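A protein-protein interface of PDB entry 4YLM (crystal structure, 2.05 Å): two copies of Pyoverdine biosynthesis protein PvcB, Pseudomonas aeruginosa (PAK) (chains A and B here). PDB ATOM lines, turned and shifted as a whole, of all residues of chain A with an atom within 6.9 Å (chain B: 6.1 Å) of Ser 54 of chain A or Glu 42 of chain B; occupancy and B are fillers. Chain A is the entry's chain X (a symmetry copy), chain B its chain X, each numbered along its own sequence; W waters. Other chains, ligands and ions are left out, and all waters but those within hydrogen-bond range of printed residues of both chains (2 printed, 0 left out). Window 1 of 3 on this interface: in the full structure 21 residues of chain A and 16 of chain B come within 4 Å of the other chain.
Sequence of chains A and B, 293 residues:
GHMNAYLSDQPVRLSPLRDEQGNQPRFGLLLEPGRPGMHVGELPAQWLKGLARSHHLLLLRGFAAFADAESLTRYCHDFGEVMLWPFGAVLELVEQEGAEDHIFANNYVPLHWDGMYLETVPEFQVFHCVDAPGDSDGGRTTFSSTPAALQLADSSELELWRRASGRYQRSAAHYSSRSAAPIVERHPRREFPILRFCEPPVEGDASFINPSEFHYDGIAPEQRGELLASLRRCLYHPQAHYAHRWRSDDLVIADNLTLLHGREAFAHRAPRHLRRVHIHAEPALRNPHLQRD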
ATOM      1  N   ARG A  26      14.346  13.026 -15.701  1.00  0.00           N
ATOM      2  CA  ARG A  26      15.189  12.694 -14.557  1.00  0.00           C
ATOM      3  C   ARG A  26      15.659  13.930 -13.772  1.00  0.00           C
ATOM      4  O   ARG A  26      16.834  14.038 -13.401  1.00  0.00           O
ATOM      5  CB  ARG A  26      16.386  11.879 -15.039  1.00  0.00           C
ATOM      6  CG  ARG A  26      16.024  10.435 -15.346  1.00  0.00           C
ATOM      7  CD  ARG A  26      17.142   9.753 -16.092  1.00  0.00           C
ATOM      8  NE  ARG A  26      17.191   8.305 -15.875  1.00  0.00           N
ATOM      9  CZ  ARG A  26      16.198   7.461 -16.147  1.00  0.00           C
ATOM     10  NH1 ARG A  26      15.045   7.909 -16.636  1.00  0.00           N
ATOM     11  NH2 ARG A  26      16.359   6.164 -15.931  1.00  0.00           N
ATOM     12  N   PHE A  27      14.732  14.854 -13.543  1.00  0.00           N
ATOM     13  CA  PHE A  27      15.004  16.058 -12.760  1.00  0.00           C
ATOM     14  C   PHE A  27      13.699  16.795 -12.563  1.00  0.00           C
ATOM     15  O   PHE A  27      12.659  16.383 -13.090  1.00  0.00           O
ATOM     16  CB  PHE A  27      16.047  16.966 -13.445  1.00  0.00           C
ATOM     17  CG  PHE A  27      15.533  17.712 -14.674  1.00  0.00           C
ATOM     18  CD1 PHE A  27      15.387  17.062 -15.890  1.00  0.00           C
ATOM     19  CD2 PHE A  27      15.250  19.071 -14.610  1.00  0.00           C
ATOM     20  CE1 PHE A  27      14.933  17.753 -17.020  1.00  0.00           C
ATOM     21  CE2 PHE A  27      14.808  19.771 -15.733  1.00  0.00           C
ATOM     22  CZ  PHE A  27      14.649  19.105 -16.942  1.00  0.00           C
ATOM     23  N   GLY A  28      13.740  17.884 -11.801  1.00  0.00           N
ATOM     24  CA  GLY A  28      12.565  18.722 -11.663  1.00  0.00           C
ATOM     25  C   GLY A  28      11.705  18.321 -10.478  1.00  0.00           C
ATOM     26  O   GLY A  28      11.627  17.152 -10.127  1.00  0.00           O
ATOM     27  N   LYS A  49      16.531  27.032  -2.371  1.00  0.00           N
ATOM     28  CA  LYS A  49      17.824  27.049  -3.052  1.00  0.00           C
ATOM     29  C   LYS A  49      18.491  25.659  -3.018  1.00  0.00           C
ATOM     30  O   LYS A  49      19.076  25.211  -4.011  1.00  0.00           O
ATOM     31  CB  LYS A  49      18.732  28.076  -2.369  1.00  0.00           C
ATOM     32  CG  LYS A  49      19.587  28.887  -3.305  1.00  0.00           C
ATOM     33  CD  LYS A  49      20.442  29.914  -2.547  1.00  0.00           C
ATOM     34  CE  LYS A  49      19.592  30.982  -1.859  1.00  0.00           C
ATOM     35  NZ  LYS A  49      20.471  32.039  -1.273  1.00  0.00           N
ATOM     36  N   GLY A  50      18.405  24.992  -1.867  1.00  0.00           N
ATOM     37  CA  GLY A  50      18.870  23.619  -1.743  1.00  0.00           C
ATOM     38  C   GLY A  50      18.174  22.684  -2.728  1.00  0.00           C
ATOM     39  O   GLY A  50      18.830  21.908  -3.424  1.00  0.00           O
ATOM     40  N   LEU A  51      16.846  22.755  -2.790  1.00  0.00           N
ATOM     41  CA  LEU A  51      16.085  21.925  -3.723  1.00  0.00           C
ATOM     42  C   LEU A  51      16.429  22.245  -5.184  1.00  0.00           C
ATOM     43  O   LEU A  51      16.539  21.338  -6.003  1.00  0.00           O
ATOM     44  CB  LEU A  51      14.576  22.092  -3.505  1.00  0.00           C
ATOM     45  CG  LEU A  51      14.006  21.653  -2.149  1.00  0.00           C
ATOM     46  CD1 LEU A  51      12.524  22.024  -2.045  1.00  0.00           C
ATOM     47  CD2 LEU A  51      14.239  20.157  -1.906  1.00  0.00           C
ATOM     48  N   ALA A  52      16.586  23.529  -5.504  1.00  0.00           N
ATOM     49  CA  ALA A  52      16.936  23.921  -6.864  1.00  0.00           C
ATOM     50  C   ALA A  52      18.286  23.344  -7.259  1.00  0.00           C
ATOM     51  O   ALA A  52      18.501  22.964  -8.409  1.00  0.00           O
ATOM     52  CB  ALA A  52      16.933  25.457  -7.020  1.00  0.00           C
ATOM     53  N   ARG A  53      19.203  23.265  -6.306  1.00  0.00           N
ATOM     54  CA  ARG A  53      20.519  22.738  -6.621  1.00  0.00           C
ATOM     55  C   ARG A  53      20.540  21.224  -6.892  1.00  0.00           C
ATOM     56  O   ARG A  53      21.384  20.743  -7.648  1.00  0.00           O
ATOM     57  CB  ARG A  53      21.518  23.116  -5.530  1.00  0.00           C
ATOM     58  CG  ARG A  53      21.955  24.559  -5.653  1.00  0.00           C
ATOM     59  CD  ARG A  53      22.655  25.051  -4.397  1.00  0.00           C
ATOM     60  NE  ARG A  53      23.215  26.381  -4.609  1.00  0.00           N
ATOM     61  CZ  ARG A  53      23.327  27.295  -3.652  1.00  0.00           C
ATOM     62  NH1 ARG A  53      22.915  27.016  -2.420  1.00  0.00           N
ATOM     63  NH2 ARG A  53      23.842  28.485  -3.932  1.00  0.00           N
ATOM     64  N   SER A  54      19.623  20.477  -6.279  1.00  0.00           N
ATOM     65  CA  SER A  54      19.640  19.012  -6.437  1.00  0.00           C
ATOM     66  C   SER A  54      18.605  18.517  -7.454  1.00  0.00           C
ATOM     67  O   SER A  54      18.828  17.520  -8.141  1.00  0.00           O
ATOM     68  CB  SER A  54      19.395  18.331  -5.091  1.00  0.00           C
ATOM     69  OG  SER A  54      18.121  18.743  -4.594  1.00  0.00           O
ATOM     70  N   HIS A  55      17.478  19.219  -7.551  1.00  0.00           N
ATOM     71  CA  HIS A  55      16.441  18.863  -8.506  1.00  0.00           C
ATOM     72  C   HIS A  55      16.563  19.686  -9.800  1.00  0.00           C
ATOM     73  O   HIS A  55      15.932  19.351 -10.798  1.00  0.00           O
ATOM     74  CB  HIS A  55      15.052  19.086  -7.910  1.00  0.00           C
ATOM     75  CG  HIS A  55      14.731  18.200  -6.740  1.00  0.00           C
ATOM     76  ND1 HIS A  55      14.313  16.894  -6.888  1.00  0.00           N
ATOM     77  CD2 HIS A  55      14.724  18.449  -5.408  1.00  0.00           C
ATOM     78  CE1 HIS A  55      14.074  16.375  -5.696  1.00  0.00           C
ATOM     79  NE2 HIS A  55      14.327  17.293  -4.780  1.00  0.00           N
ATOM     80  N   HIS A  56      17.333  20.778  -9.746  1.00  0.00           N
ATOM     81  CA  HIS A  56      17.661  21.628 -10.915  1.00  0.00           C
ATOM     82  C   HIS A  56      16.554  22.519 -11.461  1.00  0.00           C
ATOM     83  O   HIS A  56      16.830  23.574 -12.036  1.00  0.00           O
ATOM     84  CB  HIS A  56      18.315  20.803 -12.046  1.00  0.00           C
ATOM     85  CG  HIS A  56      19.446  19.950 -11.568  1.00  0.00           C
ATOM     86  ND1 HIS A  56      20.515  20.466 -10.866  1.00  0.00           N
ATOM     87  CD2 HIS A  56      19.666  18.614 -11.664  1.00  0.00           C
ATOM     88  CE1 HIS A  56      21.350  19.487 -10.556  1.00  0.00           C
ATOM     89  NE2 HIS A  56      20.858  18.353 -11.026  1.00  0.00           N
ATOM     90  N   LEU A  57      15.305  22.108 -11.303  1.00  0.00           N
ATOM     91  CA  LEU A  57      14.183  22.899 -11.791  1.00  0.00           C
ATOM     92  C   LEU A  57      13.011  22.772 -10.830  1.00  0.00           C
ATOM     93  O   LEU A  57      12.486  21.678 -10.627  1.00  0.00           O
ATOM     94  CB  LEU A  57      13.755  22.428 -13.201  1.00  0.00           C
ATOM     95  CG  LEU A  57      12.677  23.265 -13.907  1.00  0.00           C
ATOM     96  CD1 LEU A  57      13.131  24.717 -14.093  1.00  0.00           C
ATOM     97  CD2 LEU A  57      12.277  22.661 -15.270  1.00  0.00           C
ATOM     98  N   LEU A  58      12.603  23.881 -10.216  1.00  0.00           N
ATOM     99  CA  LEU A  58      11.450  23.853  -9.327  1.00  0.00           C
ATOM    100  C   LEU A  58      10.271  24.560  -9.983  1.00  0.00           C
ATOM    101  O   LEU A  58      10.429  25.632 -10.575  1.00  0.00           O
ATOM    102  CB  LEU A  58      11.756  24.555  -7.996  1.00  0.00           C
ATOM    103  CG  LEU A  58      13.055  24.194  -7.276  1.00  0.00           C
ATOM    104  CD1 LEU A  58      13.121  24.938  -5.928  1.00  0.00           C
ATOM    105  CD2 LEU A  58      13.150  22.687  -7.056  1.00  0.00           C
ATOM    106  N   SER A 145      18.355  18.734 -18.619  1.00  0.00           N
ATOM    107  CA  SER A 145      19.339  18.407 -17.587  1.00  0.00           C
ATOM    108  C   SER A 145      20.586  17.831 -18.234  1.00  0.00           C
ATOM    109  O   SER A 145      20.526  16.780 -18.870  1.00  0.00           O
ATOM    110  CB  SER A 145      18.750  17.380 -16.620  1.00  0.00           C
ATOM    111  OG  SER A 145      19.787  16.699 -15.938  1.00  0.00           O
ATOM    112  N   PRO A 147      23.311  16.563 -16.851  1.00  0.00           N
ATOM    113  CA  PRO A 147      23.725  15.263 -16.295  1.00  0.00           C
ATOM    114  C   PRO A 147      22.874  14.106 -16.819  1.00  0.00           C
ATOM    115  O   PRO A 147      23.416  13.022 -17.045  1.00  0.00           O
ATOM    116  CB  PRO A 147      23.537  15.438 -14.778  1.00  0.00           C
ATOM    117  CG  PRO A 147      23.713  16.959 -14.565  1.00  0.00           C
ATOM    118  CD  PRO A 147      23.031  17.563 -15.801  1.00  0.00           C
ATOM    119  N   GLN A 151      24.092  10.663 -19.061  1.00  0.00           N
ATOM    120  CA  GLN A 151      23.799   9.265 -18.737  1.00  0.00           C
ATOM    121  C   GLN A 151      23.223   8.522 -19.944  1.00  0.00           C
ATOM    122  O   GLN A 151      23.183   7.297 -19.961  1.00  0.00           O
ATOM    123  CB  GLN A 151      22.799   9.153 -17.577  1.00  0.00           C
ATOM    124  CG  GLN A 151      23.148   9.949 -16.323  1.00  0.00           C
ATOM    125  CD  GLN A 151      24.573   9.764 -15.881  1.00  0.00           C
ATOM    126  OE1 GLN A 151      25.018   8.644 -15.643  1.00  0.00           O
ATOM    127  NE2 GLN A 151      25.307  10.871 -15.763  1.00  0.00           N
ATOM    128  N   ARG A 190      30.401  22.778  -7.697  1.00  0.00           N
ATOM    129  CA  ARG A 190      30.081  21.518  -7.038  1.00  0.00           C
ATOM    130  C   ARG A 190      30.678  20.300  -7.732  1.00  0.00           C
ATOM    131  O   ARG A 190      30.420  19.163  -7.334  1.00  0.00           O
ATOM    132  CB  ARG A 190      28.562  21.385  -6.890  1.00  0.00           C
ATOM    133  CG  ARG A 190      27.958  22.427  -5.941  1.00  0.00           C
ATOM    134  CD  ARG A 190      26.476  22.150  -5.735  1.00  0.00           C
ATOM    135  NE  ARG A 190      25.655  22.556  -6.874  1.00  0.00           N
ATOM    136  CZ  ARG A 190      24.575  21.901  -7.284  1.00  0.00           C
ATOM    137  NH1 ARG A 190      24.218  20.775  -6.680  1.00  0.00           N
ATOM    138  NH2 ARG A 190      23.846  22.366  -8.297  1.00  0.00           N
ATOM    139  N   PHE A 192      30.469  18.186 -10.167  1.00  0.00           N
ATOM    140  CA  PHE A 192      29.931  17.055 -10.933  1.00  0.00           C
ATOM    141  C   PHE A 192      29.908  17.342 -12.431  1.00  0.00           C
ATOM    142  O   PHE A 192      29.865  18.500 -12.836  1.00  0.00           O
ATOM    143  CB  PHE A 192      28.550  16.632 -10.423  1.00  0.00           C
ATOM    144  CG  PHE A 192      27.511  17.727 -10.472  1.00  0.00           C
ATOM    145  CD1 PHE A 192      26.726  17.904 -11.598  1.00  0.00           C
ATOM    146  CD2 PHE A 192      27.309  18.563  -9.377  1.00  0.00           C
ATOM    147  CE1 PHE A 192      25.748  18.910 -11.642  1.00  0.00           C
ATOM    148  CE2 PHE A 192      26.351  19.565  -9.407  1.00  0.00           C
ATOM    149  CZ  PHE A 192      25.562  19.737 -10.539  1.00  0.00           C
ATOM    150  N   PRO A 193      29.955  16.285 -13.260  1.00  0.00           N
ATOM    151  CA  PRO A 193      29.964  16.473 -14.718  1.00  0.00           C
ATOM    152  C   PRO A 193      28.700  17.122 -15.266  1.00  0.00           C
ATOM    153  O   PRO A 193      27.577  16.729 -14.926  1.00  0.00           O
ATOM    154  CB  PRO A 193      30.106  15.037 -15.260  1.00  0.00           C
ATOM    155  CG  PRO A 193      30.807  14.296 -14.164  1.00  0.00           C
ATOM    156  CD  PRO A 193      30.236  14.884 -12.884  1.00  0.00           C
ATOM    157  N   ASP A 255      18.205  25.981 -12.237  1.00  0.00           N
ATOM    158  CA  ASP A 255      19.643  25.897 -11.991  1.00  0.00           C
ATOM    159  C   ASP A 255      20.377  26.112 -13.316  1.00  0.00           C
ATOM    160  O   ASP A 255      20.600  25.166 -14.076  1.00  0.00           O
ATOM    161  CB  ASP A 255      19.973  24.509 -11.388  1.00  0.00           C
ATOM    162  CG  ASP A 255      21.457  24.285 -11.137  1.00  0.00           C
ATOM    163  OD1 ASP A 255      22.275  25.214 -11.325  1.00  0.00           O
ATOM    164  OD2 ASP A 255      21.809  23.141 -10.731  1.00  0.00           O
ATOM    165  N   THR A 258      23.574  23.968 -14.350  1.00  0.00           N
ATOM    166  CA  THR A 258      23.417  22.550 -14.662  1.00  0.00           C
ATOM    167  C   THR A 258      22.545  22.335 -15.903  1.00  0.00           C
ATOM    168  O   THR A 258      22.818  21.455 -16.716  1.00  0.00           O
ATOM    169  CB  THR A 258      22.767  21.804 -13.480  1.00  0.00           C
ATOM    170  OG1 THR A 258      23.598  21.954 -12.321  1.00  0.00           O
ATOM    171  CG2 THR A 258      22.615  20.303 -13.793  1.00  0.00           C
ATOM    172  N   ASP B   9      13.105  15.284   1.062  1.00  0.00           N
ATOM    173  CA  ASP B   9      12.665  16.059  -0.084  1.00  0.00           C
ATOM    174  C   ASP B   9      13.808  16.177  -1.094  1.00  0.00           C
ATOM    175  O   ASP B   9      13.649  16.790  -2.145  1.00  0.00           O
ATOM    176  CB  ASP B   9      12.158  17.442   0.345  1.00  0.00           C
ATOM    177  CG  ASP B   9      12.995  18.057   1.453  1.00  0.00           C
ATOM    178  OD1 ASP B   9      14.131  17.590   1.684  1.00  0.00           O
ATOM    179  OD2 ASP B   9      12.513  19.007   2.104  1.00  0.00           O
ATOM    180  N   GLN B  10      14.955  15.586  -0.762  1.00  0.00           N
ATOM    181  CA  GLN B  10      16.116  15.569  -1.655  1.00  0.00           C
ATOM    182  C   GLN B  10      16.084  14.290  -2.510  1.00  0.00           C
ATOM    183  O   GLN B  10      15.487  13.292  -2.110  1.00  0.00           O
ATOM    184  CB  GLN B  10      17.413  15.633  -0.837  1.00  0.00           C
ATOM    185  CG  GLN B  10      17.604  16.961  -0.062  1.00  0.00           C
ATOM    186  CD  GLN B  10      17.911  18.138  -0.974  1.00  0.00           C
ATOM    187  OE1 GLN B  10      18.442  17.966  -2.076  1.00  0.00           O
ATOM    188  NE2 GLN B  10      17.588  19.341  -0.515  1.00  0.00           N
ATOM    189  N   PRO B  11      16.726  14.310  -3.688  1.00  0.00           N
ATOM    190  CA  PRO B  11      16.704  13.106  -4.548  1.00  0.00           C
ATOM    191  C   PRO B  11      17.707  12.047  -4.087  1.00  0.00           C
ATOM    192  O   PRO B  11      18.742  11.778  -4.725  1.00  0.00           O
ATOM    193  CB  PRO B  11      17.050  13.663  -5.936  1.00  0.00           C
ATOM    194  CG  PRO B  11      17.998  14.827  -5.622  1.00  0.00           C
ATOM    195  CD  PRO B  11      17.468  15.430  -4.303  1.00  0.00           C
ATOM    196  N   ARG B  35      19.177   8.935  -8.306  1.00  0.00           N
ATOM    197  CA  ARG B  35      19.183   8.876  -9.768  1.00  0.00           C
ATOM    198  C   ARG B  35      20.386   8.104 -10.257  1.00  0.00           C
ATOM    199  O   ARG B  35      21.451   8.161  -9.651  1.00  0.00           O
ATOM    200  CB  ARG B  35      19.241  10.278 -10.393  1.00  0.00           C
ATOM    201  CG  ARG B  35      18.029  11.166 -10.119  1.00  0.00           C
ATOM    202  CD  ARG B  35      18.118  12.475 -10.947  1.00  0.00           C
ATOM    203  NE  ARG B  35      19.217  13.346 -10.517  1.00  0.00           N
ATOM    204  CZ  ARG B  35      19.048  14.459  -9.800  1.00  0.00           C
ATOM    205  NH1 ARG B  35      17.830  14.829  -9.425  1.00  0.00           N
ATOM    206  NH2 ARG B  35      20.101  15.195  -9.442  1.00  0.00           N
ATOM    207  N   GLY B  37      23.743   7.321 -11.797  1.00  0.00           N
ATOM    208  CA  GLY B  37      24.936   8.109 -12.074  1.00  0.00           C
ATOM    209  C   GLY B  37      25.132   9.346 -11.200  1.00  0.00           C
ATOM    210  O   GLY B  37      26.069  10.119 -11.409  1.00  0.00           O
ATOM    211  N   MET B  38      24.265   9.538 -10.212  1.00  0.00           N
ATOM    212  CA  MET B  38      24.338  10.744  -9.381  1.00  0.00           C
ATOM    213  C   MET B  38      25.694  10.911  -8.696  1.00  0.00           C
ATOM    214  O   MET B  38      26.297   9.950  -8.221  1.00  0.00           O
ATOM    215  CB  MET B  38      23.201  10.760  -8.361  1.00  0.00           C
ATOM    216  CG  MET B  38      23.231  11.934  -7.381  1.00  0.00           C
ATOM    217  SD  MET B  38      21.747  11.904  -6.338  1.00  0.00           S
ATOM    218  CE  MET B  38      20.491  12.308  -7.515  1.00  0.00           C
ATOM    219  N   HIS B  39      26.173  12.147  -8.661  1.00  0.00           N
ATOM    220  CA  HIS B  39      27.481  12.481  -8.100  1.00  0.00           C
ATOM    221  C   HIS B  39      27.236  13.155  -6.745  1.00  0.00           C
ATOM    222  O   HIS B  39      26.197  13.774  -6.562  1.00  0.00           O
ATOM    223  CB  HIS B  39      28.152  13.452  -9.077  1.00  0.00           C
ATOM    224  CG  HIS B  39      29.568  13.800  -8.745  1.00  0.00           C
ATOM    225  ND1 HIS B  39      29.904  14.671  -7.732  1.00  0.00           N
ATOM    226  CD2 HIS B  39      30.733  13.456  -9.349  1.00  0.00           C
ATOM    227  CE1 HIS B  39      31.219  14.819  -7.700  1.00  0.00           C
ATOM    228  NE2 HIS B  39      31.744  14.095  -8.673  1.00  0.00           N
ATOM    229  N   VAL B  40      28.159  13.038  -5.792  1.00  0.00           N
ATOM    230  CA  VAL B  40      27.914  13.593  -4.468  1.00  0.00           C
ATOM    231  C   VAL B  40      27.635  15.100  -4.517  1.00  0.00           C
ATOM    232  O   VAL B  40      26.911  15.625  -3.673  1.00  0.00           O
ATOM    233  CB  VAL B  40      29.086  13.363  -3.488  1.00  0.00           C
ATOM    234  CG1 VAL B  40      29.267  11.870  -3.190  1.00  0.00           C
ATOM    235  CG2 VAL B  40      30.347  13.967  -4.038  1.00  0.00           C
ATOM    236  N   GLY B  41      28.217  15.784  -5.499  1.00  0.00           N
ATOM    237  CA  GLY B  41      28.120  17.235  -5.583  1.00  0.00           C
ATOM    238  C   GLY B  41      26.740  17.746  -5.954  1.00  0.00           C
ATOM    239  O   GLY B  41      26.431  18.924  -5.774  1.00  0.00           O
ATOM    240  N   GLU B  42      25.906  16.862  -6.481  1.00  0.00           N
ATOM    241  CA  GLU B  42      24.532  17.223  -6.818  1.00  0.00           C
ATOM    242  C   GLU B  42      23.678  17.546  -5.579  1.00  0.00           C
ATOM    243  O   GLU B  42      22.693  18.271  -5.680  1.00  0.00           O
ATOM    244  CB  GLU B  42      23.893  16.133  -7.693  1.00  0.00           C
ATOM    245  CG  GLU B  42      24.640  15.961  -9.026  1.00  0.00           C
ATOM    246  CD  GLU B  42      24.095  14.845  -9.910  1.00  0.00           C
ATOM    247  OE1 GLU B  42      22.898  14.849 -10.239  1.00  0.00           O
ATOM    248  OE2 GLU B  42      24.887  13.973 -10.300  1.00  0.00           O
ATOM    249  N   LEU B  43      24.063  17.035  -4.413  1.00  0.00           N
ATOM    250  CA  LEU B  43      23.336  17.347  -3.177  1.00  0.00           C
ATOM    251  C   LEU B  43      23.842  18.675  -2.610  1.00  0.00           C
ATOM    252  O   LEU B  43      25.007  19.012  -2.779  1.00  0.00           O
ATOM    253  CB  LEU B  43      23.532  16.220  -2.147  1.00  0.00           C
ATOM    254  CG  LEU B  43      23.092  14.827  -2.624  1.00  0.00           C
ATOM    255  CD1 LEU B  43      23.365  13.775  -1.546  1.00  0.00           C
ATOM    256  CD2 LEU B  43      21.609  14.856  -2.980  1.00  0.00           C
ATOM    257  N   PRO B  44      22.966  19.442  -1.943  1.00  0.00           N
ATOM    258  CA  PRO B  44      23.431  20.724  -1.399  1.00  0.00           C
ATOM    259  C   PRO B  44      24.254  20.544  -0.129  1.00  0.00           C
ATOM    260  O   PRO B  44      23.778  19.928   0.822  1.00  0.00           O
ATOM    261  CB  PRO B  44      22.127  21.483  -1.075  1.00  0.00           C
ATOM    262  CG  PRO B  44      20.981  20.525  -1.327  1.00  0.00           C
ATOM    263  CD  PRO B  44      21.558  19.164  -1.622  1.00  0.00           C
HETATM  264  O   HOH W   1      16.808  22.167   0.609  1.00  0.00           O
HETATM  265  O   HOH W   2      21.265  15.760 -12.270  1.00  0.00           O
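The side-chain hydroxyl (OG) of Ser 54 of chain A sits at hydrogen-bond distance from the side-chain amide oxygen (OE1) of Gln 10 of chain B (2.7 Å).
The guanidinium group (NH1) of Arg 190 of chain A sits at hydrogen-bond distance from the backbone carbonyl oxygen (O) of Gly 41 of chain B (3.0 Å).
NH2 of Arg 35 of chain B is in hydrogen-bond range of O of Ser 54 of chain A (3.0 Å).
O of Asp 9 of chain B sits at hydrogen-bond distance from NE2 of His 55 of chain A (2.8 Å).
O of Glu 42 of chain B lies close to O of Arg 53 of chain A, 3.4 Å away.
The guanidinium group of Arg 190 of chain A is in hydrogen-bond range of the backbone carbonyl oxygen of Glu 42 of chain B.
The side-chain hydroxyl (OG) of Ser 54 of chain A sits at hydrogen-bond distance from the backbone carbonyl oxygen (O) of Gly 50 of chain A (3.4 Å).
The backbone carbonyl oxygen (O) of Pro 147 of chain A lies within hydrogen-bond range of the side-chain amide nitrogen (NE2) of Gln 151 of chain A (3.1 Å).
O of Arg 53 of chain A lies close to ND1 of His 56 of chain A (3.3 Å).
N of Gly 28 of chain A lies within hydrogen-bond range of O of His 55 of chain A, at 2.8 Å.
N of His 39 of chain B lies within hydrogen-bond range of OE2 of Glu 42 of chain B, at 2.8 Å.
OE1 of Glu 42 of chain B lies within salt-bridge range of NH2 of Arg 35 of chain B, 2.9 Å away.
Among the printed residues, merely in contact across the chains: Arg 26 of chain A with Arg 35 of chain B, Gly 50 of chain A with Pro 44 of chain B, Leu 51 of chain A with Asp 9 of chain B, Leu 51 of chain A with Gln 10 of chain B, Ser 54 of chain A with Pro 11 of chain B, Ser 54 of chain A with Glu 42 of chain B, His 55 of chain A with Gln 10 of chain B, His 55 of chain A with Pro 11 of chain B, His 56 of chain A with Arg 35 of chain B, Gln 151 of chain A with Gly 37 of chain B, Phe 192 of chain A with His 39 of chain B, Phe 192 of chain A with Gly 41 of chain B, Phe 192 of chain A with Glu 42 of chain B and Pro 193 of chain A with His 39 of chain B.
Of chain B, only Gln 10 (2.7 Å), Pro 11 (3.4 Å), Arg 35 (3.0 Å) and Glu 42 (3.2 Å) come within 4 Å of Ser 54 of chain A.
Glu 42 of chain B touches just these residues of chain A: Arg 53, Ser 54, Arg 190 and Phe 192.
Printed residues of chain A within 4 Å of Gly 41 of chain B: Arg 190 and Phe 192.
Of the printed residues of chain B, Leu 51 of chain A touches Asp 9 (3.4 Å) and Gln 10 (3.7 Å).
Of the printed residues of chain B, Arg 26 of chain A touches Arg 35 (3.2 Å).
Of the printed residues of chain B, Phe 192 of chain A touches His 39 (3.4 Å), Gly 41 (3.6 Å) and Glu 42 (3.6 Å).
The nearest residue of chain A that does not touch Glu 42 of chain B is His 56 of chain A (4.1 Å).
The nearest printed residue of chain B that does not touch His 56 of chain A is Glu 42 of chain B (4.1 Å).
Of the 21 printed residues of chain A, 11 touch a printed residue of chain B.
Hydrophobic or aromatic side chains of chain A within 4 Å of the printed part of chain B: Leu 51, His 55, His 56, Phe 192 and Pro 193.
Of the 12 printed residues of chain B, 9 touch a printed residue of chain A.
Hydrophobic or aromatic side chains of chain B that line the printed part of chain A: Pro 11, His 39 and Pro 44.
Among the printed residues, 20 pairs touch across the chains.
Among the printed residues, no Asp or Glu carboxylate lies within 4 Å of a Lys or Arg side-chain nitrogen of the other chain.
No position is printed for both chains.
Water W2 lies within hydrogen-bond range of OE1 of Glu 42 of chain B (2.8 Å), NE2 of His 56 of chain A (2.9 Å) and NH2 of Arg 35 of chain B (3.1 Å).
Water W1 lies within hydrogen-bond range of NE2 of Gln 10 of chain B (3.1 Å) and N of Leu 51 of chain A (3.4 Å).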
